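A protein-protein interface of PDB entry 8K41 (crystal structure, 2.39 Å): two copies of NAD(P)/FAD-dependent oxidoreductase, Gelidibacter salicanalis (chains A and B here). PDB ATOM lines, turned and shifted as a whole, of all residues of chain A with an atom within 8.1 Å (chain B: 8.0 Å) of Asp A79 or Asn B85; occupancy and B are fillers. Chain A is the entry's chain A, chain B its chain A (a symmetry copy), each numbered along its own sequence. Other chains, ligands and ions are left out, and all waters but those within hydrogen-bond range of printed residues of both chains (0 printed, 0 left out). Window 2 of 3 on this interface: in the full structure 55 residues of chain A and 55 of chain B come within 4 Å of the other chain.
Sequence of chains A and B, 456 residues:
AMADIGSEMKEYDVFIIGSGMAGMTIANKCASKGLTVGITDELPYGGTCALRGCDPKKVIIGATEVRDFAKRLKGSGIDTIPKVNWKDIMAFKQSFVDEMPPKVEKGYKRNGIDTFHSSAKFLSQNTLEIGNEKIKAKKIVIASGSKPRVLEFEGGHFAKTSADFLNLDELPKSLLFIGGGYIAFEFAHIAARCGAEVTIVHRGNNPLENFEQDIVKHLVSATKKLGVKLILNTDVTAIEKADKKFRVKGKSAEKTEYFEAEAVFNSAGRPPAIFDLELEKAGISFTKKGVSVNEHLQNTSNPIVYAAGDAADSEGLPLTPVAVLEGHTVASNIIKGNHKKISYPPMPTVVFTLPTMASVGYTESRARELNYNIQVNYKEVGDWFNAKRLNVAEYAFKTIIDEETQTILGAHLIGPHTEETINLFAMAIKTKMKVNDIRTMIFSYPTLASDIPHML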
ATOM      1  N   ALA A  70      29.863 -19.277   4.637  1.00  0.00           N
ATOM      2  CA  ALA A  70      29.819 -18.685   3.274  1.00  0.00           C
ATOM      3  C   ALA A  70      28.911 -19.499   2.347  1.00  0.00           C
ATOM      4  O   ALA A  70      28.104 -18.870   1.640  1.00  0.00           O
ATOM      5  CB  ALA A  70      31.199 -18.576   2.679  1.00  0.00           C
ATOM      6  N   LEU A  73      25.208 -18.741   3.115  1.00  0.00           N
ATOM      7  CA  LEU A  73      24.613 -17.436   2.714  1.00  0.00           C
ATOM      8  C   LEU A  73      24.949 -17.133   1.246  1.00  0.00           C
ATOM      9  O   LEU A  73      24.871 -15.953   0.877  1.00  0.00           O
ATOM     10  CB  LEU A  73      25.135 -16.326   3.631  1.00  0.00           C
ATOM     11  CG  LEU A  73      24.594 -16.300   5.059  1.00  0.00           C
ATOM     12  CD1 LEU A  73      25.073 -15.059   5.804  1.00  0.00           C
ATOM     13  CD2 LEU A  73      23.085 -16.368   5.076  1.00  0.00           C
ATOM     14  N   LYS A  74      25.296 -18.143   0.437  1.00  0.00           N
ATOM     15  CA  LYS A  74      25.669 -17.929  -0.984  1.00  0.00           C
ATOM     16  C   LYS A  74      24.488 -17.265  -1.699  1.00  0.00           C
ATOM     17  O   LYS A  74      23.391 -17.818  -1.629  1.00  0.00           O
ATOM     18  CB  LYS A  74      26.040 -19.247  -1.672  1.00  0.00           C
ATOM     19  CG  LYS A  74      26.345 -19.123  -3.156  1.00  0.00           C
ATOM     20  CD  LYS A  74      27.560 -18.258  -3.451  1.00  0.00           C
ATOM     21  CE  LYS A  74      27.488 -17.555  -4.791  1.00  0.00           C
ATOM     22  NZ  LYS A  74      27.821 -18.489  -5.889  1.00  0.00           N
ATOM     23  N   GLY A  75      24.702 -16.119  -2.347  1.00  0.00           N
ATOM     24  CA  GLY A  75      23.651 -15.419  -3.114  1.00  0.00           C
ATOM     25  C   GLY A  75      22.798 -14.513  -2.235  1.00  0.00           C
ATOM     26  O   GLY A  75      22.182 -13.581  -2.788  1.00  0.00           O
ATOM     27  N   SER A  76      22.761 -14.765  -0.921  1.00  0.00           N
ATOM     28  CA  SER A  76      22.056 -13.940   0.100  1.00  0.00           C
ATOM     29  C   SER A  76      22.949 -12.808   0.617  1.00  0.00           C
ATOM     30  O   SER A  76      22.522 -12.134   1.556  1.00  0.00           O
ATOM     31  CB  SER A  76      21.602 -14.781   1.250  1.00  0.00           C
ATOM     32  OG  SER A  76      20.751 -15.800   0.790  1.00  0.00           O
ATOM     33  N   GLY A  77      24.149 -12.623   0.064  1.00  0.00           N
ATOM     34  CA  GLY A  77      25.051 -11.545   0.509  1.00  0.00           C
ATOM     35  C   GLY A  77      26.511 -11.926   0.419  1.00  0.00           C
ATOM     36  O   GLY A  77      27.356 -11.043   0.658  1.00  0.00           O
ATOM     37  N   ILE A  78      26.794 -13.197   0.131  1.00  0.00           N
ATOM     38  CA  ILE A  78      28.163 -13.751  -0.087  1.00  0.00           C
ATOM     39  C   ILE A  78      28.174 -14.315  -1.506  1.00  0.00           C
ATOM     40  O   ILE A  78      27.147 -14.919  -1.911  1.00  0.00           O
ATOM     41  CB  ILE A  78      28.509 -14.814   0.983  1.00  0.00           C
ATOM     42  CG1 ILE A  78      28.253 -14.312   2.410  1.00  0.00           C
ATOM     43  CG2 ILE A  78      29.935 -15.327   0.826  1.00  0.00           C
ATOM     44  CD1 ILE A  78      29.108 -13.120   2.852  1.00  0.00           C
ATOM     45  N   ASP A  79      29.255 -14.073  -2.248  1.00  0.00           N
ATOM     46  CA  ASP A  79      29.346 -14.385  -3.699  1.00  0.00           C
ATOM     47  C   ASP A  79      30.545 -15.315  -3.975  1.00  0.00           C
ATOM     48  O   ASP A  79      30.727 -15.712  -5.152  1.00  0.00           O
ATOM     49  CB  ASP A  79      29.346 -13.076  -4.496  1.00  0.00           C
ATOM     50  CG  ASP A  79      27.982 -12.391  -4.562  1.00  0.00           C
ATOM     51  OD1 ASP A  79      26.954 -13.105  -4.590  1.00  0.00           O
ATOM     52  OD2 ASP A  79      27.955 -11.148  -4.598  1.00  0.00           O
ATOM     53  N   THR A  80      31.306 -15.702  -2.943  1.00  0.00           N
ATOM     54  CA  THR A  80      32.499 -16.586  -3.053  1.00  0.00           C
ATOM     55  C   THR A  80      32.563 -17.512  -1.822  1.00  0.00           C
ATOM     56  O   THR A  80      32.430 -17.010  -0.680  1.00  0.00           O
ATOM     57  CB  THR A  80      33.769 -15.745  -3.230  1.00  0.00           C
ATOM     58  OG1 THR A  80      33.650 -14.684  -2.282  1.00  0.00           O
ATOM     59  CG2 THR A  80      33.954 -15.152  -4.613  1.00  0.00           C
ATOM     60  N   ILE A  81      32.741 -18.817  -2.055  1.00  0.00           N
ATOM     61  CA  ILE A  81      32.912 -19.879  -1.019  1.00  0.00           C
ATOM     62  C   ILE A  81      34.390 -20.273  -1.005  1.00  0.00           C
ATOM     63  O   ILE A  81      34.864 -20.949  -1.920  1.00  0.00           O
ATOM     64  CB  ILE A  81      32.003 -21.098  -1.304  1.00  0.00           C
ATOM     65  CG1 ILE A  81      30.568 -20.691  -1.655  1.00  0.00           C
ATOM     66  CG2 ILE A  81      32.041 -22.071  -0.132  1.00  0.00           C
ATOM     67  CD1 ILE A  81      29.730 -21.794  -2.261  1.00  0.00           C
ATOM     68  N   PRO A  82      35.162 -19.921   0.049  1.00  0.00           N
ATOM     69  CA  PRO A  82      36.586 -20.235   0.078  1.00  0.00           C
ATOM     70  C   PRO A  82      36.858 -21.748   0.103  1.00  0.00           C
ATOM     71  O   PRO A  82      36.148 -22.449   0.811  1.00  0.00           O
ATOM     72  CB  PRO A  82      37.092 -19.606   1.383  1.00  0.00           C
ATOM     73  CG  PRO A  82      35.980 -18.690   1.840  1.00  0.00           C
ATOM     74  CD  PRO A  82      34.705 -19.289   1.296  1.00  0.00           C
ATOM     75  N   ALA B  63      26.214 -11.631   7.349  1.00  0.00           N
ATOM     76  CA  ALA B  63      27.075 -11.632   6.137  1.00  0.00           C
ATOM     77  C   ALA B  63      28.422 -11.001   6.467  1.00  0.00           C
ATOM     78  O   ALA B  63      29.406 -11.330   5.798  1.00  0.00           O
ATOM     79  CB  ALA B  63      26.433 -10.901   4.990  1.00  0.00           C
ATOM     80  N   VAL B  66      30.832 -13.406   8.160  1.00  0.00           N
ATOM     81  CA  VAL B  66      31.517 -14.249   7.135  1.00  0.00           C
ATOM     82  C   VAL B  66      32.838 -13.593   6.724  1.00  0.00           C
ATOM     83  O   VAL B  66      33.863 -14.299   6.735  1.00  0.00           O
ATOM     84  CB  VAL B  66      30.584 -14.502   5.937  1.00  0.00           C
ATOM     85  CG1 VAL B  66      31.290 -15.251   4.819  1.00  0.00           C
ATOM     86  CG2 VAL B  66      29.323 -15.236   6.384  1.00  0.00           C
ATOM     87  N   PRO B  82      35.662 -12.553   1.363  1.00  0.00           N
ATOM     88  CA  PRO B  82      34.538 -12.118   0.540  1.00  0.00           C
ATOM     89  C   PRO B  82      34.167 -10.644   0.777  1.00  0.00           C
ATOM     90  O   PRO B  82      34.173 -10.227   1.927  1.00  0.00           O
ATOM     91  CB  PRO B  82      33.371 -13.014   0.979  1.00  0.00           C
ATOM     92  CG  PRO B  82      34.004 -14.122   1.788  1.00  0.00           C
ATOM     93  CD  PRO B  82      35.259 -13.532   2.384  1.00  0.00           C
ATOM     94  N   LYS B  83      33.916  -9.906  -0.313  1.00  0.00           N
ATOM     95  CA  LYS B  83      33.152  -8.631  -0.320  1.00  0.00           C
ATOM     96  C   LYS B  83      31.721  -9.017   0.043  1.00  0.00           C
ATOM     97  O   LYS B  83      31.317 -10.140  -0.321  1.00  0.00           O
ATOM     98  CB  LYS B  83      33.235  -7.941  -1.693  1.00  0.00           C
ATOM     99  CG  LYS B  83      32.454  -6.634  -1.859  1.00  0.00           C
ATOM    100  CD  LYS B  83      33.294  -5.386  -1.651  1.00  0.00           C
ATOM    101  CE  LYS B  83      32.494  -4.165  -1.246  1.00  0.00           C
ATOM    102  NZ  LYS B  83      33.374  -3.116  -0.674  1.00  0.00           N
ATOM    103  N   VAL B  84      31.003  -8.152   0.764  1.00  0.00           N
ATOM    104  CA  VAL B  84      29.554  -8.351   1.054  1.00  0.00           C
ATOM    105  C   VAL B  84      28.772  -7.714  -0.091  1.00  0.00           C
ATOM    106  O   VAL B  84      29.114  -6.594  -0.477  1.00  0.00           O
ATOM    107  CB  VAL B  84      29.170  -7.789   2.433  1.00  0.00           C
ATOM    108  CG1 VAL B  84      27.661  -7.777   2.662  1.00  0.00           C
ATOM    109  CG2 VAL B  84      29.870  -8.577   3.522  1.00  0.00           C
ATOM    110  N   ASN B  85      27.795  -8.449  -0.621  1.00  0.00           N
ATOM    111  CA  ASN B  85      26.892  -8.037  -1.724  1.00  0.00           C
ATOM    112  C   ASN B  85      25.697  -7.328  -1.092  1.00  0.00           C
ATOM    113  O   ASN B  85      24.741  -8.021  -0.667  1.00  0.00           O
ATOM    114  CB  ASN B  85      26.466  -9.246  -2.548  1.00  0.00           C
ATOM    115  CG  ASN B  85      25.544  -8.904  -3.697  1.00  0.00           C
ATOM    116  OD1 ASN B  85      24.707  -8.001  -3.598  1.00  0.00           O
ATOM    117  ND2 ASN B  85      25.671  -9.662  -4.773  1.00  0.00           N
ATOM    118  N   TRP B  86      25.770  -6.002  -1.005  1.00  0.00           N
ATOM    119  CA  TRP B  86      24.780  -5.183  -0.269  1.00  0.00           C
ATOM    120  C   TRP B  86      23.364  -5.560  -0.718  1.00  0.00           C
ATOM    121  O   TRP B  86      22.536  -5.956   0.142  1.00  0.00           O
ATOM    122  CB  TRP B  86      25.061  -3.686  -0.434  1.00  0.00           C
ATOM    123  CG  TRP B  86      24.184  -2.870   0.464  1.00  0.00           C
ATOM    124  CD1 TRP B  86      23.099  -2.131   0.098  1.00  0.00           C
ATOM    125  CD2 TRP B  86      24.251  -2.789   1.902  1.00  0.00           C
ATOM    126  NE1 TRP B  86      22.511  -1.568   1.200  1.00  0.00           N
ATOM    127  CE2 TRP B  86      23.195  -1.950   2.319  1.00  0.00           C
ATOM    128  CE3 TRP B  86      25.113  -3.316   2.874  1.00  0.00           C
ATOM    129  CZ2 TRP B  86      22.979  -1.628   3.659  1.00  0.00           C
ATOM    130  CZ3 TRP B  86      24.901  -2.995   4.197  1.00  0.00           C
ATOM    131  CH2 TRP B  86      23.850  -2.160   4.583  1.00  0.00           C
ATOM    132  N   LYS B  87      23.079  -5.441  -2.013  1.00  0.00           N
ATOM    133  CA  LYS B  87      21.721  -5.716  -2.553  1.00  0.00           C
ATOM    134  C   LYS B  87      21.231  -7.053  -1.983  1.00  0.00           C
ATOM    135  O   LYS B  87      20.169  -7.049  -1.328  1.00  0.00           O
ATOM    136  CB  LYS B  87      21.725  -5.737  -4.085  1.00  0.00           C
ATOM    137  CG  LYS B  87      21.512  -4.386  -4.753  1.00  0.00           C
ATOM    138  CD  LYS B  87      21.908  -4.393  -6.221  1.00  0.00           C
ATOM    139  CE  LYS B  87      21.362  -3.218  -7.006  1.00  0.00           C
ATOM    140  NZ  LYS B  87      20.005  -3.505  -7.526  1.00  0.00           N
ATOM    141  N   ASP B  88      22.001  -8.127  -2.209  1.00  0.00           N
ATOM    142  CA  ASP B  88      21.615  -9.531  -1.913  1.00  0.00           C
ATOM    143  C   ASP B  88      21.243  -9.654  -0.430  1.00  0.00           C
ATOM    144  O   ASP B  88      20.155 -10.209  -0.133  1.00  0.00           O
ATOM    145  CB  ASP B  88      22.711 -10.518  -2.331  1.00  0.00           C
ATOM    146  CG  ASP B  88      22.834 -10.714  -3.843  1.00  0.00           C
ATOM    147  OD1 ASP B  88      22.136  -9.986  -4.595  1.00  0.00           O
ATOM    148  OD2 ASP B  88      23.634 -11.578  -4.267  1.00  0.00           O
ATOM    149  N   ILE B  89      22.074  -9.135   0.471  1.00  0.00           N
ATOM    150  CA  ILE B  89      21.787  -9.245   1.930  1.00  0.00           C
ATOM    151  C   ILE B  89      20.613  -8.355   2.325  1.00  0.00           C
ATOM    152  O   ILE B  89      19.787  -8.870   3.131  1.00  0.00           O
ATOM    153  CB  ILE B  89      22.994  -8.992   2.840  1.00  0.00           C
ATOM    154  CG1 ILE B  89      22.561  -9.294   4.276  1.00  0.00           C
ATOM    155  CG2 ILE B  89      23.579  -7.594   2.694  1.00  0.00           C
ATOM    156  CD1 ILE B  89      23.694  -9.315   5.203  1.00  0.00           C
ATOM    157  N   MET B  90      20.518  -7.128   1.785  1.00  0.00           N
ATOM    158  CA  MET B  90      19.306  -6.267   1.956  1.00  0.00           C
ATOM    159  C   MET B  90      18.068  -7.072   1.560  1.00  0.00           C
ATOM    160  O   MET B  90      17.066  -7.070   2.330  1.00  0.00           O
ATOM    161  CB  MET B  90      19.323  -4.990   1.100  1.00  0.00           C
ATOM    162  CG  MET B  90      19.705  -3.724   1.861  1.00  0.00           C
ATOM    163  SD  MET B  90      18.596  -3.166   3.220  1.00  0.00           S
ATOM    164  CE  MET B  90      16.989  -3.611   2.579  1.00  0.00           C
ATOM    165  N   ALA B  91      18.119  -7.705   0.390  1.00  0.00           N
ATOM    166  CA  ALA B  91      16.971  -8.436  -0.198  1.00  0.00           C
ATOM    167  C   ALA B  91      16.609  -9.579   0.753  1.00  0.00           C
ATOM    168  O   ALA B  91      15.419  -9.741   1.049  1.00  0.00           O
ATOM    169  CB  ALA B  91      17.313  -8.928  -1.584  1.00  0.00           C
ATOM    170  N   PHE B  92      17.623 -10.291   1.245  1.00  0.00           N
ATOM    171  CA  PHE B  92      17.495 -11.410   2.218  1.00  0.00           C
ATOM    172  C   PHE B  92      16.879 -10.874   3.512  1.00  0.00           C
ATOM    173  O   PHE B  92      15.909 -11.421   4.005  1.00  0.00           O
ATOM    174  CB  PHE B  92      18.857 -12.071   2.474  1.00  0.00           C
ATOM    175  CG  PHE B  92      18.791 -13.311   3.329  1.00  0.00           C
ATOM    176  CD1 PHE B  92      17.743 -14.214   3.201  1.00  0.00           C
ATOM    177  CD2 PHE B  92      19.776 -13.590   4.263  1.00  0.00           C
ATOM    178  CE1 PHE B  92      17.688 -15.370   3.970  1.00  0.00           C
ATOM    179  CE2 PHE B  92      19.712 -14.738   5.045  1.00  0.00           C
ATOM    180  CZ  PHE B  92      18.662 -15.624   4.903  1.00  0.00           C
ATOM    181  N   ASP B 169      19.157   0.888  -0.447  1.00  0.00           N
ATOM    182  CA  ASP B 169      19.334   0.118  -1.714  1.00  0.00           C
ATOM    183  C   ASP B 169      20.820  -0.050  -2.016  1.00  0.00           C
ATOM    184  O   ASP B 169      21.221  -1.100  -2.564  1.00  0.00           O
ATOM    185  CB  ASP B 169      18.754   0.838  -2.931  1.00  0.00           C
ATOM    186  CG  ASP B 169      17.267   1.047  -2.820  1.00  0.00           C
ATOM    187  OD1 ASP B 169      16.551   0.037  -2.745  1.00  0.00           O
ATOM    188  OD2 ASP B 169      16.852   2.213  -2.771  1.00  0.00           O
ATOM    189  N   CYS B 194      31.375  -3.500   5.048  1.00  0.00           N
ATOM    190  CA  CYS B 194      30.789  -3.528   3.678  1.00  0.00           C
ATOM    191  C   CYS B 194      31.466  -2.504   2.748  1.00  0.00           C
ATOM    192  O   CYS B 194      31.061  -2.428   1.567  1.00  0.00           O
ATOM    193  CB  CYS B 194      29.284  -3.335   3.768  1.00  0.00           C
ATOM    194  SG  CYS B 194      28.466  -4.744   4.574  1.00  0.00           S
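Along chain A the printed residues that touch a printed residue of chain B span positions 70 to 80. Of the 15 printed residues of chain B, 8 touch a printed residue of chain A. Printed residues of chain B that touch a printed residue of chain A: Ala B63, Val B66, Pro B82, Val B84, Asn B85, Asp B88, Ile B89 and Phe B92. Hydrophobic or aromatic side chains of chain B that line the printed part of chain A: Val B66, Pro B82, Val B84, Ile B89 and Phe B92. Among the printed residues, no Asp or Glu carboxylate lies within 4 Å of a Lys or Arg side-chain nitrogen of the other chain.
Of the printed residues of chain B, Asp A79 touches Asn B85 and Asp B88. Of chain A, only Gly A77 (2.9 Å) and Asp A79 (2.7 Å) come within 4 Å of Asn B85. Of the printed residues of chain A, Ala B63 touches Leu A73 (3.9 Å) and Ile A78 (3.5 Å). Of the printed residues of chain A, Val B84 touches Gly A77 (3.5 Å). Of the printed residues of chain B, Gly A75 touches Asp B88 (2.9 Å). Of the printed residues of chain A, Pro B82 touches Thr A80.
Val B66 touches Ala A70 (CG1 to CB, 3.96 Å). CD1 of Leu A73 touches N of Ala B63 (3.9 Å). Phe B92 touches Leu A73 (CE2 to CD2, 3.7 Å). Ser A76 touches Phe B92 (CB to CD2, 3.7 Å). Gly A77 touches Val B84. Gly A77 touches Asp B88. N of Ile B89 touches CA of Gly A77, at 3.8 Å. Ile A78 touches Ala B63. Ile A78 touches Val B66 (CD1 to CG1, 3.6 Å). CB of Pro B82 touches OG1 of Thr A80, 3.7 Å away.
The backbone NH (N) of Ile A78 sits at hydrogen-bond distance from the backbone carbonyl oxygen (O) of Leu A73 (3.4 Å). The side-chain amide oxygen (OD1) of Asn B85 lies close to the backbone NH (N) of Lys B87, 3.4 Å away. The side-chain carboxylate (OD2) of Asp B88 lies within hydrogen-bond range of the side-chain amide nitrogen (ND2) of Asn B85, 2.8 Å away.
The backbone carbonyl oxygen of Ser A76 sits close to the backbone NH of Ile B89, at 3.2 Å. N of Asn B85 lies within hydrogen-bond range of O of Gly A77 (2.9 Å). The side-chain carboxylate (OD2) of Asp A79 lies within hydrogen-bond range of the side-chain amide nitrogen (ND2) of Asn B85, 2.7 Å away. The backbone carbonyl oxygen (O) of Gly A75 lies close to the side-chain carboxylate (OD2) of Asp B88, 2.9 Å away. O of Ser A76 lies close to O of Asp B88 (3.5 Å).
Position printed for both chains: 82. Of the 16 pairs that touch across the chains among the printed residues, none has its exchanged pair printed and touching as well.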
